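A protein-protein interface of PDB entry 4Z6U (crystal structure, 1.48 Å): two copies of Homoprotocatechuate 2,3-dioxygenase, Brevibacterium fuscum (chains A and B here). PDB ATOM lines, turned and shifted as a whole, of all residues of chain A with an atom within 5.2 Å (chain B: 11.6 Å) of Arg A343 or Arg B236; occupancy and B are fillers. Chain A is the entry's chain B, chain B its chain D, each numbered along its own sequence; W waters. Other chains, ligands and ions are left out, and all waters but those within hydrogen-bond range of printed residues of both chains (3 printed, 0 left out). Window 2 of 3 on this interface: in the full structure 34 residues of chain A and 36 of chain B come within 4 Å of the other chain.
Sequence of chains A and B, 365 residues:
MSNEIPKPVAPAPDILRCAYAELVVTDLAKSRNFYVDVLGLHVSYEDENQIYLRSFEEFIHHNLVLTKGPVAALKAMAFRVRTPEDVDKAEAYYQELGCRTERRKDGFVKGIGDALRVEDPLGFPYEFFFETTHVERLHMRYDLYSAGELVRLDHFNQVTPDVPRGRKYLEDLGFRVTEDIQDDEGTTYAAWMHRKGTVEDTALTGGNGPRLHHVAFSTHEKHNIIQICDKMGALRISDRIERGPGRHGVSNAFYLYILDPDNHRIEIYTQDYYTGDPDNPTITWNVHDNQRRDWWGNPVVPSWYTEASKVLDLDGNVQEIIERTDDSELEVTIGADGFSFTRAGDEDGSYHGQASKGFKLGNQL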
ATOM      1  N   TRP A 285       3.619  11.779 -18.859  1.00  0.00           N
ATOM      2  CA  TRP A 285       3.584  10.363 -18.625  1.00  0.00           C
ATOM      3  C   TRP A 285       3.781  10.080 -17.138  1.00  0.00           C
ATOM      4  O   TRP A 285       4.549  10.786 -16.439  1.00  0.00           O
ATOM      5  CB  TRP A 285       4.713   9.686 -19.395  1.00  0.00           C
ATOM      6  CG  TRP A 285       4.680   9.856 -20.854  1.00  0.00           C
ATOM      7  CD1 TRP A 285       5.032  10.969 -21.551  1.00  0.00           C
ATOM      8  CD2 TRP A 285       4.274   8.876 -21.836  1.00  0.00           C
ATOM      9  NE1 TRP A 285       4.869  10.764 -22.883  1.00  0.00           N
ATOM     10  CE2 TRP A 285       4.421   9.489 -23.104  1.00  0.00           C
ATOM     11  CE3 TRP A 285       3.847   7.555 -21.768  1.00  0.00           C
ATOM     12  CZ2 TRP A 285       4.164   8.820 -24.307  1.00  0.00           C
ATOM     13  CZ3 TRP A 285       3.557   6.882 -22.967  1.00  0.00           C
ATOM     14  CH2 TRP A 285       3.710   7.524 -24.220  1.00  0.00           C
ATOM     15  N   ASP A 289       4.516   3.976 -15.928  1.00  0.00           N
ATOM     16  CA  ASP A 289       4.017   3.471 -17.214  1.00  0.00           C
ATOM     17  C   ASP A 289       5.212   2.868 -17.971  1.00  0.00           C
ATOM     18  O   ASP A 289       6.128   3.590 -18.408  1.00  0.00           O
ATOM     19  CB  ASP A 289       3.408   4.649 -17.994  1.00  0.00           C
ATOM     20  CG  ASP A 289       2.816   4.266 -19.333  1.00  0.00           C
ATOM     21  OD1 ASP A 289       3.177   3.221 -19.898  1.00  0.00           O
ATOM     22  OD2 ASP A 289       1.962   5.070 -19.826  1.00  0.00           O
ATOM     23  N   GLN A 291       5.499   1.880 -20.917  1.00  0.00           N
ATOM     24  CA  GLN A 291       5.632   2.317 -22.314  1.00  0.00           C
ATOM     25  C   GLN A 291       6.149   3.743 -22.484  1.00  0.00           C
ATOM     26  O   GLN A 291       6.202   4.248 -23.596  1.00  0.00           O
ATOM     27  CB  GLN A 291       4.311   2.122 -23.091  1.00  0.00           C
ATOM     28  CG  GLN A 291       3.874   0.662 -23.164  1.00  0.00           C
ATOM     29  CD  GLN A 291       2.667   0.336 -24.015  1.00  0.00           C
ATOM     30  OE1 GLN A 291       2.199  -0.820 -24.069  1.00  0.00           O
ATOM     31  NE2 GLN A 291       2.185   1.304 -24.746  1.00  0.00           N
ATOM     32  N   TRP A 295       8.345   2.397 -25.851  1.00  0.00           N
ATOM     33  CA  TRP A 295       6.933   2.185 -26.176  1.00  0.00           C
ATOM     34  C   TRP A 295       6.588   0.701 -26.278  1.00  0.00           C
ATOM     35  O   TRP A 295       5.440   0.310 -26.056  1.00  0.00           O
ATOM     36  CB  TRP A 295       6.644   2.870 -27.517  1.00  0.00           C
ATOM     37  CG  TRP A 295       5.267   2.825 -28.075  1.00  0.00           C
ATOM     38  CD1 TRP A 295       4.897   2.302 -29.283  1.00  0.00           C
ATOM     39  CD2 TRP A 295       4.065   3.397 -27.506  1.00  0.00           C
ATOM     40  NE1 TRP A 295       3.583   2.524 -29.505  1.00  0.00           N
ATOM     41  CE2 TRP A 295       3.046   3.205 -28.435  1.00  0.00           C
ATOM     42  CE3 TRP A 295       3.782   4.088 -26.311  1.00  0.00           C
ATOM     43  CZ2 TRP A 295       1.728   3.665 -28.217  1.00  0.00           C
ATOM     44  CZ3 TRP A 295       2.469   4.533 -26.110  1.00  0.00           C
ATOM     45  CH2 TRP A 295       1.476   4.305 -27.054  1.00  0.00           C
ATOM     46  N   PHE A 341       3.673  -0.718 -14.895  1.00  0.00           N
ATOM     47  CA  PHE A 341       2.501  -1.296 -15.528  1.00  0.00           C
ATOM     48  C   PHE A 341       2.536  -1.202 -17.034  1.00  0.00           C
ATOM     49  O   PHE A 341       3.151  -0.318 -17.601  1.00  0.00           O
ATOM     50  CB  PHE A 341       1.210  -0.682 -14.967  1.00  0.00           C
ATOM     51  CG  PHE A 341       1.037   0.780 -15.245  1.00  0.00           C
ATOM     52  CD1 PHE A 341       0.580   1.206 -16.487  1.00  0.00           C
ATOM     53  CD2 PHE A 341       1.345   1.740 -14.266  1.00  0.00           C
ATOM     54  CE1 PHE A 341       0.394   2.593 -16.728  1.00  0.00           C
ATOM     55  CE2 PHE A 341       1.174   3.102 -14.503  1.00  0.00           C
ATOM     56  CZ  PHE A 341       0.688   3.526 -15.742  1.00  0.00           C
ATOM     57  N   THR A 342       1.827  -2.140 -17.668  1.00  0.00           N
ATOM     58  CA  THR A 342       1.524  -2.038 -19.072  1.00  0.00           C
ATOM     59  C   THR A 342       0.205  -1.311 -19.329  1.00  0.00           C
ATOM     60  O   THR A 342       0.139  -0.443 -20.211  1.00  0.00           O
ATOM     61  CB  THR A 342       1.517  -3.435 -19.757  1.00  0.00           C
ATOM     62  OG1 THR A 342       2.774  -4.107 -19.550  1.00  0.00           O
ATOM     63  CG2 THR A 342       1.253  -3.321 -21.218  1.00  0.00           C
ATOM     64  N   ARG A 343      -0.827  -1.686 -18.572  1.00  0.00           N
ATOM     65  CA  ARG A 343      -2.154  -1.090 -18.646  1.00  0.00           C
ATOM     66  C   ARG A 343      -2.463  -0.602 -17.231  1.00  0.00           C
ATOM     67  O   ARG A 343      -2.380  -1.375 -16.265  1.00  0.00           O
ATOM     68  CB  ARG A 343      -3.210  -2.090 -19.119  1.00  0.00           C
ATOM     69  CG  ARG A 343      -3.074  -2.598 -20.547  1.00  0.00           C
ATOM     70  CD  ARG A 343      -3.812  -3.870 -20.778  1.00  0.00           C
ATOM     71  NE  ARG A 343      -3.226  -4.995 -20.088  1.00  0.00           N
ATOM     72  CZ  ARG A 343      -2.216  -5.730 -20.529  1.00  0.00           C
ATOM     73  NH1 ARG A 343      -1.647  -5.511 -21.706  1.00  0.00           N
ATOM     74  NH2 ARG A 343      -1.777  -6.695 -19.768  1.00  0.00           N
ATOM     75  N   ALA A 344      -2.728   0.690 -17.104  1.00  0.00           N
ATOM     76  CA  ALA A 344      -3.051   1.291 -15.813  1.00  0.00           C
ATOM     77  C   ALA A 344      -4.195   0.519 -15.175  1.00  0.00           C
ATOM     78  O   ALA A 344      -5.209   0.199 -15.825  1.00  0.00           O
ATOM     79  CB  ALA A 344      -3.446   2.756 -15.983  1.00  0.00           C
ATOM     80  N   GLY A 345      -3.969   0.163 -13.913  1.00  0.00           N
ATOM     81  CA  GLY A 345      -4.931  -0.571 -13.118  1.00  0.00           C
ATOM     82  C   GLY A 345      -5.009  -2.074 -13.361  1.00  0.00           C
ATOM     83  O   GLY A 345      -5.794  -2.775 -12.706  1.00  0.00           O
ATOM     84  N   ASP A 346      -4.229  -2.582 -14.307  1.00  0.00           N
ATOM     85  CA  ASP A 346      -4.189  -4.026 -14.601  1.00  0.00           C
ATOM     86  C   ASP A 346      -2.962  -4.676 -13.973  1.00  0.00           C
ATOM     87  O   ASP A 346      -1.795  -4.304 -14.253  1.00  0.00           O
ATOM     88  CB  ASP A 346      -4.205  -4.244 -16.110  1.00  0.00           C
ATOM     89  CG  ASP A 346      -4.489  -5.687 -16.533  1.00  0.00           C
ATOM     90  OD1 ASP A 346      -4.590  -6.596 -15.677  1.00  0.00           O
ATOM     91  OD2 ASP A 346      -4.570  -5.901 -17.777  1.00  0.00           O
ATOM     92  N   ASP A 348      -2.147  -7.752 -14.601  1.00  0.00           N
ATOM     93  CA  ASP A 348      -1.570  -8.505 -15.692  1.00  0.00           C
ATOM     94  C   ASP A 348      -0.669  -7.568 -16.519  1.00  0.00           C
ATOM     95  O   ASP A 348      -1.114  -6.494 -16.929  1.00  0.00           O
ATOM     96  CB  ASP A 348      -2.721  -9.092 -16.529  1.00  0.00           C
ATOM     97  CG  ASP A 348      -2.249  -9.891 -17.694  1.00  0.00           C
ATOM     98  OD1 ASP A 348      -1.303 -10.669 -17.527  1.00  0.00           O
ATOM     99  OD2 ASP A 348      -2.834  -9.771 -18.776  1.00  0.00           O
ATOM    100  N   GLY A 349       0.589  -7.954 -16.741  1.00  0.00           N
ATOM    101  CA  GLY A 349       1.538  -7.094 -17.465  1.00  0.00           C
ATOM    102  C   GLY A 349       2.178  -6.035 -16.563  1.00  0.00           C
ATOM    103  O   GLY A 349       2.834  -5.100 -17.062  1.00  0.00           O
ATOM    104  N   LYS B  30     -10.784 -14.676 -29.435  1.00  0.00           N
ATOM    105  CA  LYS B  30      -9.593 -13.954 -28.976  1.00  0.00           C
ATOM    106  C   LYS B  30      -8.397 -14.200 -29.885  1.00  0.00           C
ATOM    107  O   LYS B  30      -7.636 -13.276 -30.225  1.00  0.00           O
ATOM    108  CB  LYS B  30      -9.262 -14.316 -27.552  1.00  0.00           C
ATOM    109  CG  LYS B  30     -10.205 -13.671 -26.568  1.00  0.00           C
ATOM    110  CD  LYS B  30      -9.623 -13.694 -25.171  1.00  0.00           C
ATOM    111  CE  LYS B  30     -10.681 -13.353 -24.124  1.00  0.00           C
ATOM    112  NZ  LYS B  30     -10.229 -13.861 -22.789  1.00  0.00           N
ATOM    113  N   ASN B  33      -8.915 -12.157 -33.036  1.00  0.00           N
ATOM    114  CA  ASN B  33      -8.547 -10.769 -32.843  1.00  0.00           C
ATOM    115  C   ASN B  33      -7.036 -10.571 -33.025  1.00  0.00           C
ATOM    116  O   ASN B  33      -6.603  -9.612 -33.642  1.00  0.00           O
ATOM    117  CB  ASN B  33      -9.005 -10.287 -31.493  1.00  0.00           C
ATOM    118  CG  ASN B  33      -8.558  -8.853 -31.192  1.00  0.00           C
ATOM    119  OD1 ASN B  33      -7.660  -8.639 -30.364  1.00  0.00           O
ATOM    120  ND2 ASN B  33      -9.168  -7.863 -31.874  1.00  0.00           N
ATOM    121  N   PHE B  34      -6.246 -11.507 -32.504  1.00  0.00           N
ATOM    122  CA  PHE B  34      -4.812 -11.401 -32.589  1.00  0.00           C
ATOM    123  C   PHE B  34      -4.331 -11.570 -34.024  1.00  0.00           C
ATOM    124  O   PHE B  34      -3.553 -10.710 -34.532  1.00  0.00           O
ATOM    125  CB  PHE B  34      -4.162 -12.437 -31.670  1.00  0.00           C
ATOM    126  CG  PHE B  34      -2.658 -12.375 -31.620  1.00  0.00           C
ATOM    127  CD1 PHE B  34      -2.021 -11.437 -30.841  1.00  0.00           C
ATOM    128  CD2 PHE B  34      -1.876 -13.299 -32.307  1.00  0.00           C
ATOM    129  CE1 PHE B  34      -0.631 -11.388 -30.793  1.00  0.00           C
ATOM    130  CE2 PHE B  34      -0.504 -13.266 -32.239  1.00  0.00           C
ATOM    131  CZ  PHE B  34       0.119 -12.305 -31.483  1.00  0.00           C
ATOM    132  N   VAL B  38      -4.983  -7.751 -35.099  1.00  0.00           N
ATOM    133  CA  VAL B  38      -3.675  -7.189 -34.761  1.00  0.00           C
ATOM    134  C   VAL B  38      -2.683  -7.406 -35.912  1.00  0.00           C
ATOM    135  O   VAL B  38      -2.072  -6.457 -36.382  1.00  0.00           O
ATOM    136  CB  VAL B  38      -3.132  -7.669 -33.428  1.00  0.00           C
ATOM    137  CG1 VAL B  38      -1.750  -7.063 -33.105  1.00  0.00           C
ATOM    138  CG2 VAL B  38      -4.155  -7.399 -32.312  1.00  0.00           C
ATOM    139  N   GLN B 227       6.574  -1.502 -37.186  1.00  0.00           N
ATOM    140  CA  GLN B 227       5.167  -1.171 -37.080  1.00  0.00           C
ATOM    141  C   GLN B 227       4.380  -2.155 -36.225  1.00  0.00           C
ATOM    142  O   GLN B 227       3.491  -1.750 -35.482  1.00  0.00           O
ATOM    143  CB  GLN B 227       4.505  -1.053 -38.455  1.00  0.00           C
ATOM    144  CG  GLN B 227       2.982  -1.125 -38.459  1.00  0.00           C
ATOM    145  CD  GLN B 227       2.283  -0.001 -37.760  1.00  0.00           C
ATOM    146  OE1 GLN B 227       2.869   1.029 -37.401  1.00  0.00           O
ATOM    147  NE2 GLN B 227       0.994  -0.184 -37.580  1.00  0.00           N
ATOM    148  N   ILE B 228       4.675  -3.453 -36.357  1.00  0.00           N
ATOM    149  CA  ILE B 228       3.965  -4.403 -35.500  1.00  0.00           C
ATOM    150  C   ILE B 228       4.194  -4.051 -34.013  1.00  0.00           C
ATOM    151  O   ILE B 228       3.250  -4.065 -33.207  1.00  0.00           O
ATOM    152  CB  ILE B 228       4.394  -5.850 -35.813  1.00  0.00           C
ATOM    153  CG1 ILE B 228       3.946  -6.220 -37.251  1.00  0.00           C
ATOM    154  CG2 ILE B 228       3.812  -6.816 -34.801  1.00  0.00           C
ATOM    155  CD1 ILE B 228       4.608  -7.495 -37.747  1.00  0.00           C
ATOM    156  N   CYS B 229       5.444  -3.762 -33.658  1.00  0.00           N
ATOM    157  CA  CYS B 229       5.770  -3.311 -32.326  1.00  0.00           C
ATOM    158  C   CYS B 229       4.998  -2.039 -31.925  1.00  0.00           C
ATOM    159  O   CYS B 229       4.413  -1.960 -30.828  1.00  0.00           O
ATOM    160  CB  CYS B 229       7.263  -3.033 -32.154  1.00  0.00           C
ATOM    161  SG  CYS B 229       8.304  -4.462 -32.418  1.00  0.00           S
ATOM    162  N   ASP B 230       5.021  -1.079 -32.824  1.00  0.00           N
ATOM    163  CA  ASP B 230       4.373   0.196 -32.589  1.00  0.00           C
ATOM    164  C   ASP B 230       2.867  -0.019 -32.369  1.00  0.00           C
ATOM    165  O   ASP B 230       2.260   0.608 -31.487  1.00  0.00           O
ATOM    166  CB  ASP B 230       4.583   1.140 -33.743  1.00  0.00           C
ATOM    167  CG  ASP B 230       6.012   1.667 -33.830  1.00  0.00           C
ATOM    168  OD1 ASP B 230       6.725   1.748 -32.800  1.00  0.00           O
ATOM    169  OD2 ASP B 230       6.414   2.050 -34.950  1.00  0.00           O
ATOM    170  N   LYS B 231       2.267  -0.895 -33.184  1.00  0.00           N
ATOM    171  CA  LYS B 231       0.838  -1.172 -33.104  1.00  0.00           C
ATOM    172  C   LYS B 231       0.508  -1.848 -31.766  1.00  0.00           C
ATOM    173  O   LYS B 231      -0.506  -1.512 -31.112  1.00  0.00           O
ATOM    174  CB  LYS B 231       0.377  -2.037 -34.259  1.00  0.00           C
ATOM    175  CG  LYS B 231      -1.130  -2.228 -34.277  1.00  0.00           C
ATOM    176  CD  LYS B 231      -1.590  -2.927 -35.533  1.00  0.00           C
ATOM    177  CE  LYS B 231      -3.076  -3.155 -35.543  1.00  0.00           C
ATOM    178  NZ  LYS B 231      -3.502  -3.839 -36.812  1.00  0.00           N
ATOM    179  N   MET B 232       1.357  -2.796 -31.362  1.00  0.00           N
ATOM    180  CA  MET B 232       1.157  -3.476 -30.063  1.00  0.00           C
ATOM    181  C   MET B 232       1.289  -2.483 -28.900  1.00  0.00           C
ATOM    182  O   MET B 232       0.523  -2.562 -27.924  1.00  0.00           O
ATOM    183  CB  MET B 232       2.065  -4.692 -29.926  1.00  0.00           C
ATOM    184  CG  MET B 232       1.653  -5.774 -30.889  1.00  0.00           C
ATOM    185  SD  MET B 232       2.721  -7.202 -30.920  1.00  0.00           S
ATOM    186  CE  MET B 232       2.231  -7.995 -29.407  1.00  0.00           C
ATOM    187  N   GLY B 233       2.183  -1.491 -29.034  1.00  0.00           N
ATOM    188  CA  GLY B 233       2.224  -0.437 -28.008  1.00  0.00           C
ATOM    189  C   GLY B 233       0.907   0.381 -27.987  1.00  0.00           C
ATOM    190  O   GLY B 233       0.343   0.659 -26.919  1.00  0.00           O
ATOM    191  N   ALA B 234       0.399   0.737 -29.166  1.00  0.00           N
ATOM    192  CA  ALA B 234      -0.824   1.542 -29.245  1.00  0.00           C
ATOM    193  C   ALA B 234      -2.033   0.777 -28.677  1.00  0.00           C
ATOM    194  O   ALA B 234      -2.948   1.368 -28.091  1.00  0.00           O
ATOM    195  CB  ALA B 234      -1.081   1.940 -30.681  1.00  0.00           C
ATOM    196  N   LEU B 235      -2.049  -0.530 -28.920  1.00  0.00           N
ATOM    197  CA  LEU B 235      -3.081  -1.425 -28.362  1.00  0.00           C
ATOM    198  C   LEU B 235      -2.858  -1.763 -26.894  1.00  0.00           C
ATOM    199  O   LEU B 235      -3.697  -2.484 -26.304  1.00  0.00           O
ATOM    200  CB  LEU B 235      -3.218  -2.706 -29.211  1.00  0.00           C
ATOM    201  CG  LEU B 235      -3.718  -2.460 -30.629  1.00  0.00           C
ATOM    202  CD1 LEU B 235      -3.629  -3.738 -31.441  1.00  0.00           C
ATOM    203  CD2 LEU B 235      -5.115  -1.915 -30.594  1.00  0.00           C
ATOM    204  N   ARG B 236      -1.758  -1.275 -26.306  1.00  0.00           N
ATOM    205  CA  ARG B 236      -1.436  -1.506 -24.911  1.00  0.00           C
ATOM    206  C   ARG B 236      -1.313  -2.987 -24.602  1.00  0.00           C
ATOM    207  O   ARG B 236      -1.733  -3.464 -23.539  1.00  0.00           O
ATOM    208  CB  ARG B 236      -2.419  -0.756 -23.987  1.00  0.00           C
ATOM    209  CG  ARG B 236      -2.097   0.725 -23.904  1.00  0.00           C
ATOM    210  CD  ARG B 236      -0.968   1.030 -22.926  1.00  0.00           C
ATOM    211  NE  ARG B 236      -0.514   2.413 -22.972  1.00  0.00           N
ATOM    212  CZ  ARG B 236       0.474   2.894 -22.217  1.00  0.00           C
ATOM    213  NH1 ARG B 236       1.046   2.125 -21.306  1.00  0.00           N
ATOM    214  NH2 ARG B 236       0.893   4.164 -22.380  1.00  0.00           N
ATOM    215  N   ILE B 237      -0.690  -3.696 -25.542  1.00  0.00           N
ATOM    216  CA  ILE B 237      -0.371  -5.130 -25.408  1.00  0.00           C
ATOM    217  C   ILE B 237       1.130  -5.362 -25.598  1.00  0.00           C
ATOM    218  O   ILE B 237       1.570  -6.417 -26.058  1.00  0.00           O
ATOM    219  CB  ILE B 237      -1.228  -6.041 -26.322  1.00  0.00           C
ATOM    220  CG1 ILE B 237      -1.065  -5.701 -27.792  1.00  0.00           C
ATOM    221  CG2 ILE B 237      -2.713  -5.989 -25.889  1.00  0.00           C
ATOM    222  CD1 ILE B 237      -1.812  -6.606 -28.740  1.00  0.00           C
ATOM    223  N   SER B 238       1.918  -4.367 -25.215  1.00  0.00           N
ATOM    224  CA  SER B 238       3.371  -4.498 -25.295  1.00  0.00           C
ATOM    225  C   SER B 238       3.948  -5.632 -24.472  1.00  0.00           C
ATOM    226  O   SER B 238       5.041  -6.107 -24.763  1.00  0.00           O
ATOM    227  CB  SER B 238       4.083  -3.205 -24.939  1.00  0.00           C
ATOM    228  OG  SER B 238       3.792  -2.757 -23.642  1.00  0.00           O
ATOM    229  N   ASP B 239       3.215  -6.060 -23.442  1.00  0.00           N
ATOM    230  CA  ASP B 239       3.597  -7.229 -22.685  1.00  0.00           C
ATOM    231  C   ASP B 239       3.585  -8.526 -23.494  1.00  0.00           C
ATOM    232  O   ASP B 239       4.162  -9.515 -23.069  1.00  0.00           O
ATOM    233  CB  ASP B 239       2.768  -7.387 -21.374  1.00  0.00           C
ATOM    234  CG  ASP B 239       1.264  -7.385 -21.571  1.00  0.00           C
ATOM    235  OD1 ASP B 239       0.728  -6.816 -22.546  1.00  0.00           O
ATOM    236  OD2 ASP B 239       0.610  -7.968 -20.681  1.00  0.00           O
ATOM    237  N   ARG B 240       2.948  -8.518 -24.635  1.00  0.00           N
ATOM    238  CA  ARG B 240       2.967  -9.672 -25.549  1.00  0.00           C
ATOM    239  C   ARG B 240       4.097  -9.613 -26.588  1.00  0.00           C
ATOM    240  O   ARG B 240       4.212 -10.519 -27.429  1.00  0.00           O
ATOM    241  CB  ARG B 240       1.619  -9.813 -26.231  1.00  0.00           C
ATOM    242  CG  ARG B 240       0.425  -9.741 -25.256  1.00  0.00           C
ATOM    243  CD  ARG B 240       0.526 -10.749 -24.141  1.00  0.00           C
ATOM    244  NE  ARG B 240       0.344 -12.116 -24.668  1.00  0.00           N
ATOM    245  CZ  ARG B 240       0.549 -13.229 -23.951  1.00  0.00           C
ATOM    246  NH1 ARG B 240       1.072 -13.139 -22.719  1.00  0.00           N
ATOM    247  NH2 ARG B 240       0.268 -14.425 -24.450  1.00  0.00           N
ATOM    248  N   ILE B 241       4.907  -8.561 -26.539  1.00  0.00           N
ATOM    249  CA  ILE B 241       6.179  -8.547 -27.268  1.00  0.00           C
ATOM    250  C   ILE B 241       7.191  -9.240 -26.345  1.00  0.00           C
ATOM    251  O   ILE B 241       7.498  -8.744 -25.242  1.00  0.00           O
ATOM    252  CB  ILE B 241       6.648  -7.128 -27.553  1.00  0.00           C
ATOM    253  CG1 ILE B 241       5.612  -6.378 -28.419  1.00  0.00           C
ATOM    254  CG2 ILE B 241       8.063  -7.156 -28.163  1.00  0.00           C
ATOM    255  CD1 ILE B 241       5.954  -4.902 -28.593  1.00  0.00           C
ATOM    256  N   LEU B 259       3.714 -13.119 -28.640  1.00  0.00           N
ATOM    257  CA  LEU B 259       2.994 -14.228 -28.071  1.00  0.00           C
ATOM    258  C   LEU B 259       1.506 -14.088 -28.325  1.00  0.00           C
ATOM    259  O   LEU B 259       0.927 -13.039 -28.040  1.00  0.00           O
ATOM    260  CB  LEU B 259       3.263 -14.280 -26.543  1.00  0.00           C
ATOM    261  CG  LEU B 259       4.717 -14.439 -26.118  1.00  0.00           C
ATOM    262  CD1 LEU B 259       4.854 -14.247 -24.612  1.00  0.00           C
ATOM    263  CD2 LEU B 259       5.273 -15.764 -26.567  1.00  0.00           C
ATOM    264  N   ASP B 260       0.882 -15.122 -28.871  1.00  0.00           N
ATOM    265  CA  ASP B 260      -0.561 -15.109 -29.115  1.00  0.00           C
ATOM    266  C   ASP B 260      -1.342 -15.365 -27.803  1.00  0.00           C
ATOM    267  O   ASP B 260      -0.751 -15.547 -26.731  1.00  0.00           O
ATOM    268  CB  ASP B 260      -0.930 -16.074 -30.271  1.00  0.00           C
ATOM    269  CG  ASP B 260      -1.304 -17.507 -29.832  1.00  0.00           C
ATOM    270  OD1 ASP B 260      -1.104 -17.909 -28.664  1.00  0.00           O
ATOM    271  OD2 ASP B 260      -1.777 -18.278 -30.736  1.00  0.00           O
ATOM    272  N   PRO B 261      -2.679 -15.326 -27.870  1.00  0.00           N
ATOM    273  CA  PRO B 261      -3.461 -15.453 -26.628  1.00  0.00           C
ATOM    274  C   PRO B 261      -3.275 -16.743 -25.818  1.00  0.00           C
ATOM    275  O   PRO B 261      -3.503 -16.746 -24.584  1.00  0.00           O
ATOM    276  CB  PRO B 261      -4.885 -15.303 -27.118  1.00  0.00           C
ATOM    277  CG  PRO B 261      -4.762 -14.401 -28.316  1.00  0.00           C
ATOM    278  CD  PRO B 261      -3.521 -14.882 -29.000  1.00  0.00           C
ATOM    279  N   ASN B 263      -0.231 -18.161 -25.684  1.00  0.00           N
ATOM    280  CA  ASN B 263       1.228 -18.157 -25.564  1.00  0.00           C
ATOM    281  C   ASN B 263       1.975 -18.857 -26.690  1.00  0.00           C
ATOM    282  O   ASN B 263       3.184 -19.050 -26.566  1.00  0.00           O
ATOM    283  CB  ASN B 263       1.655 -18.722 -24.208  1.00  0.00           C
ATOM    284  CG  ASN B 263       1.015 -17.988 -23.061  1.00  0.00           C
ATOM    285  OD1 ASN B 263       0.823 -16.774 -23.121  1.00  0.00           O
ATOM    286  ND2 ASN B 263       0.670 -18.711 -22.020  1.00  0.00           N
HETATM  287  O   HOH W   1       4.937  -3.367 -21.163  1.00  0.00           O
HETATM  288  O   HOH W   2      -1.757  -8.571 -22.746  1.00  0.00           O
HETATM  289  O   HOH W   3      -0.824   4.707 -19.496  1.00  0.00           O
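The guanidinium group (NH1) of Arg B236 is in salt-bridge range of the side-chain carboxylate (OD1) of Asp A289.
The backbone carbonyl oxygen (O) of Gly B233 lies within hydrogen-bond range of the side-chain amide nitrogen (NE2) of Gln A291 (2.9 Å).
NE2 of Gln A291 sits close to NE of Arg B236 (3.4 Å).
OE1 of Gln A291 lies within hydrogen-bond range of OG of Ser B238 (2.5 Å).
NE1 of Trp A295 sits at hydrogen-bond distance from O of Asp B230, 3.1 Å away.
The backbone carbonyl oxygen (O) of Thr A342 sits at hydrogen-bond distance from the guanidinium group (NH1) of Arg B236 (2.9 Å).
The guanidinium group (NH1) of Arg A343 sits at hydrogen-bond distance from the backbone carbonyl oxygen (O) of Arg B236, at 2.7 Å.
The side-chain carboxylate (OD1) of Asp B239 lies within salt-bridge range of the guanidinium group (NH1) of Arg A343 (2.8 Å).
The side-chain carboxylate of Asp A289 lies within hydrogen-bond range of the backbone NH of Gln A291, at 2.9 Å.
The side-chain hydroxyl (OG1) of Thr A342 is in hydrogen-bond range of the backbone carbonyl oxygen (O) of Gly A349 (2.7 Å).
The guanidinium group (NE) of Arg A343 is in salt-bridge range of the side-chain carboxylate (OD2) of Asp A346 (2.8 Å).
The backbone NH of Ile B237 sits at hydrogen-bond distance from the backbone carbonyl oxygen of Met B232 (2.9 Å).
Arg B236 touches Trp A285 (NH2 to CZ3, 3.9 Å).
Trp A295 touches Gly B233.
Ala B234 touches Trp A295 (N to CZ2, 3.4 Å).
Trp A295 touches Ser B238 (O to CB, 3.9 Å).
Ser B238 touches Thr A342.
Thr A342 touches Asp B239 (OG1 to CB, 3.8 Å).
Ile B237 touches Arg A343 (CA to NH1, 3.9 Å).
Asp B239 touches Gly A349 (OD2 to CA, 3.5 Å).
Arg B236 touches just these residues of chain A: Trp A285 (3.9 Å), Asp A289 (2.8 Å), Gln A291 (3.4 Å), Thr A342 (2.9 Å) and Arg A343 (2.7 Å).
Asp A289 touches just one residue of chain B: Arg B236.
Gln A291 touches three residues of chain B.
No residue of chain B comes within 4 Å of Phe A341.
No residue of chain B comes within 4 Å of Ala A344.
No residue of chain B comes within 4 Å of Asp A346.
Gly A349 touches one residue of chain B.
Of the printed residues of chain B, Trp A295 touches Asp B230, Gly B233, Ala B234 and Ser B238.
Printed residues of chain B within 4 Å of Trp A285: Arg B236 (3.9 Å).
Of the printed residues of chain A, Ser B238 touches Gln A291 (2.5 Å), Trp A295 (3.9 Å) and Thr A342 (3.6 Å).
Asp A348 touches none of the printed residues of chain B.
The nearest residue of chain B that does not touch Arg A343 is Ser B238 (5.1 Å).
The nearest residue of chain A that does not touch Arg B236 is Trp A295 (4.1 Å).
The nearest printed residue of chain B that does not touch Trp A285 is Gly B233 (8.0 Å).
Printed residues of chain B that touch a printed residue of chain A: Asp B230, Gly B233, Ala B234, Arg B236, Ile B237, Ser B238 and Asp B239.
Along chain B the printed residues that touch a printed residue of chain A span positions 230 to 239.
Hydrophobic or aromatic side chains of chain A that line the printed part of chain B: Trp A285 and Trp A295.
Among the printed residues, Asp or Glu carboxylates within 4 Å of a Lys or Arg side-chain nitrogen of the other chain: Asp A289 with Arg B236 and Arg A343 with Asp B239.
No position is printed for both chains.
Of the 16 pairs that touch across the chains among the printed residues, none has its exchanged pair printed and touching as well.
Water W1 lies within hydrogen-bond range of the side-chain hydroxyl of Thr A342 (2.8 Å) and the side-chain hydroxyl of Ser B238 (2.8 Å).
Water W3 lies within hydrogen-bond range of the side-chain carboxylate (OD2) of Asp A289 (2.8 Å) and the guanidinium group (NH2) of Arg B236 (3.4 Å).
Water W2 bridges the side-chain carboxylate (OD1) of Asp B239 and the guanidinium group (NH1) of Arg A343.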
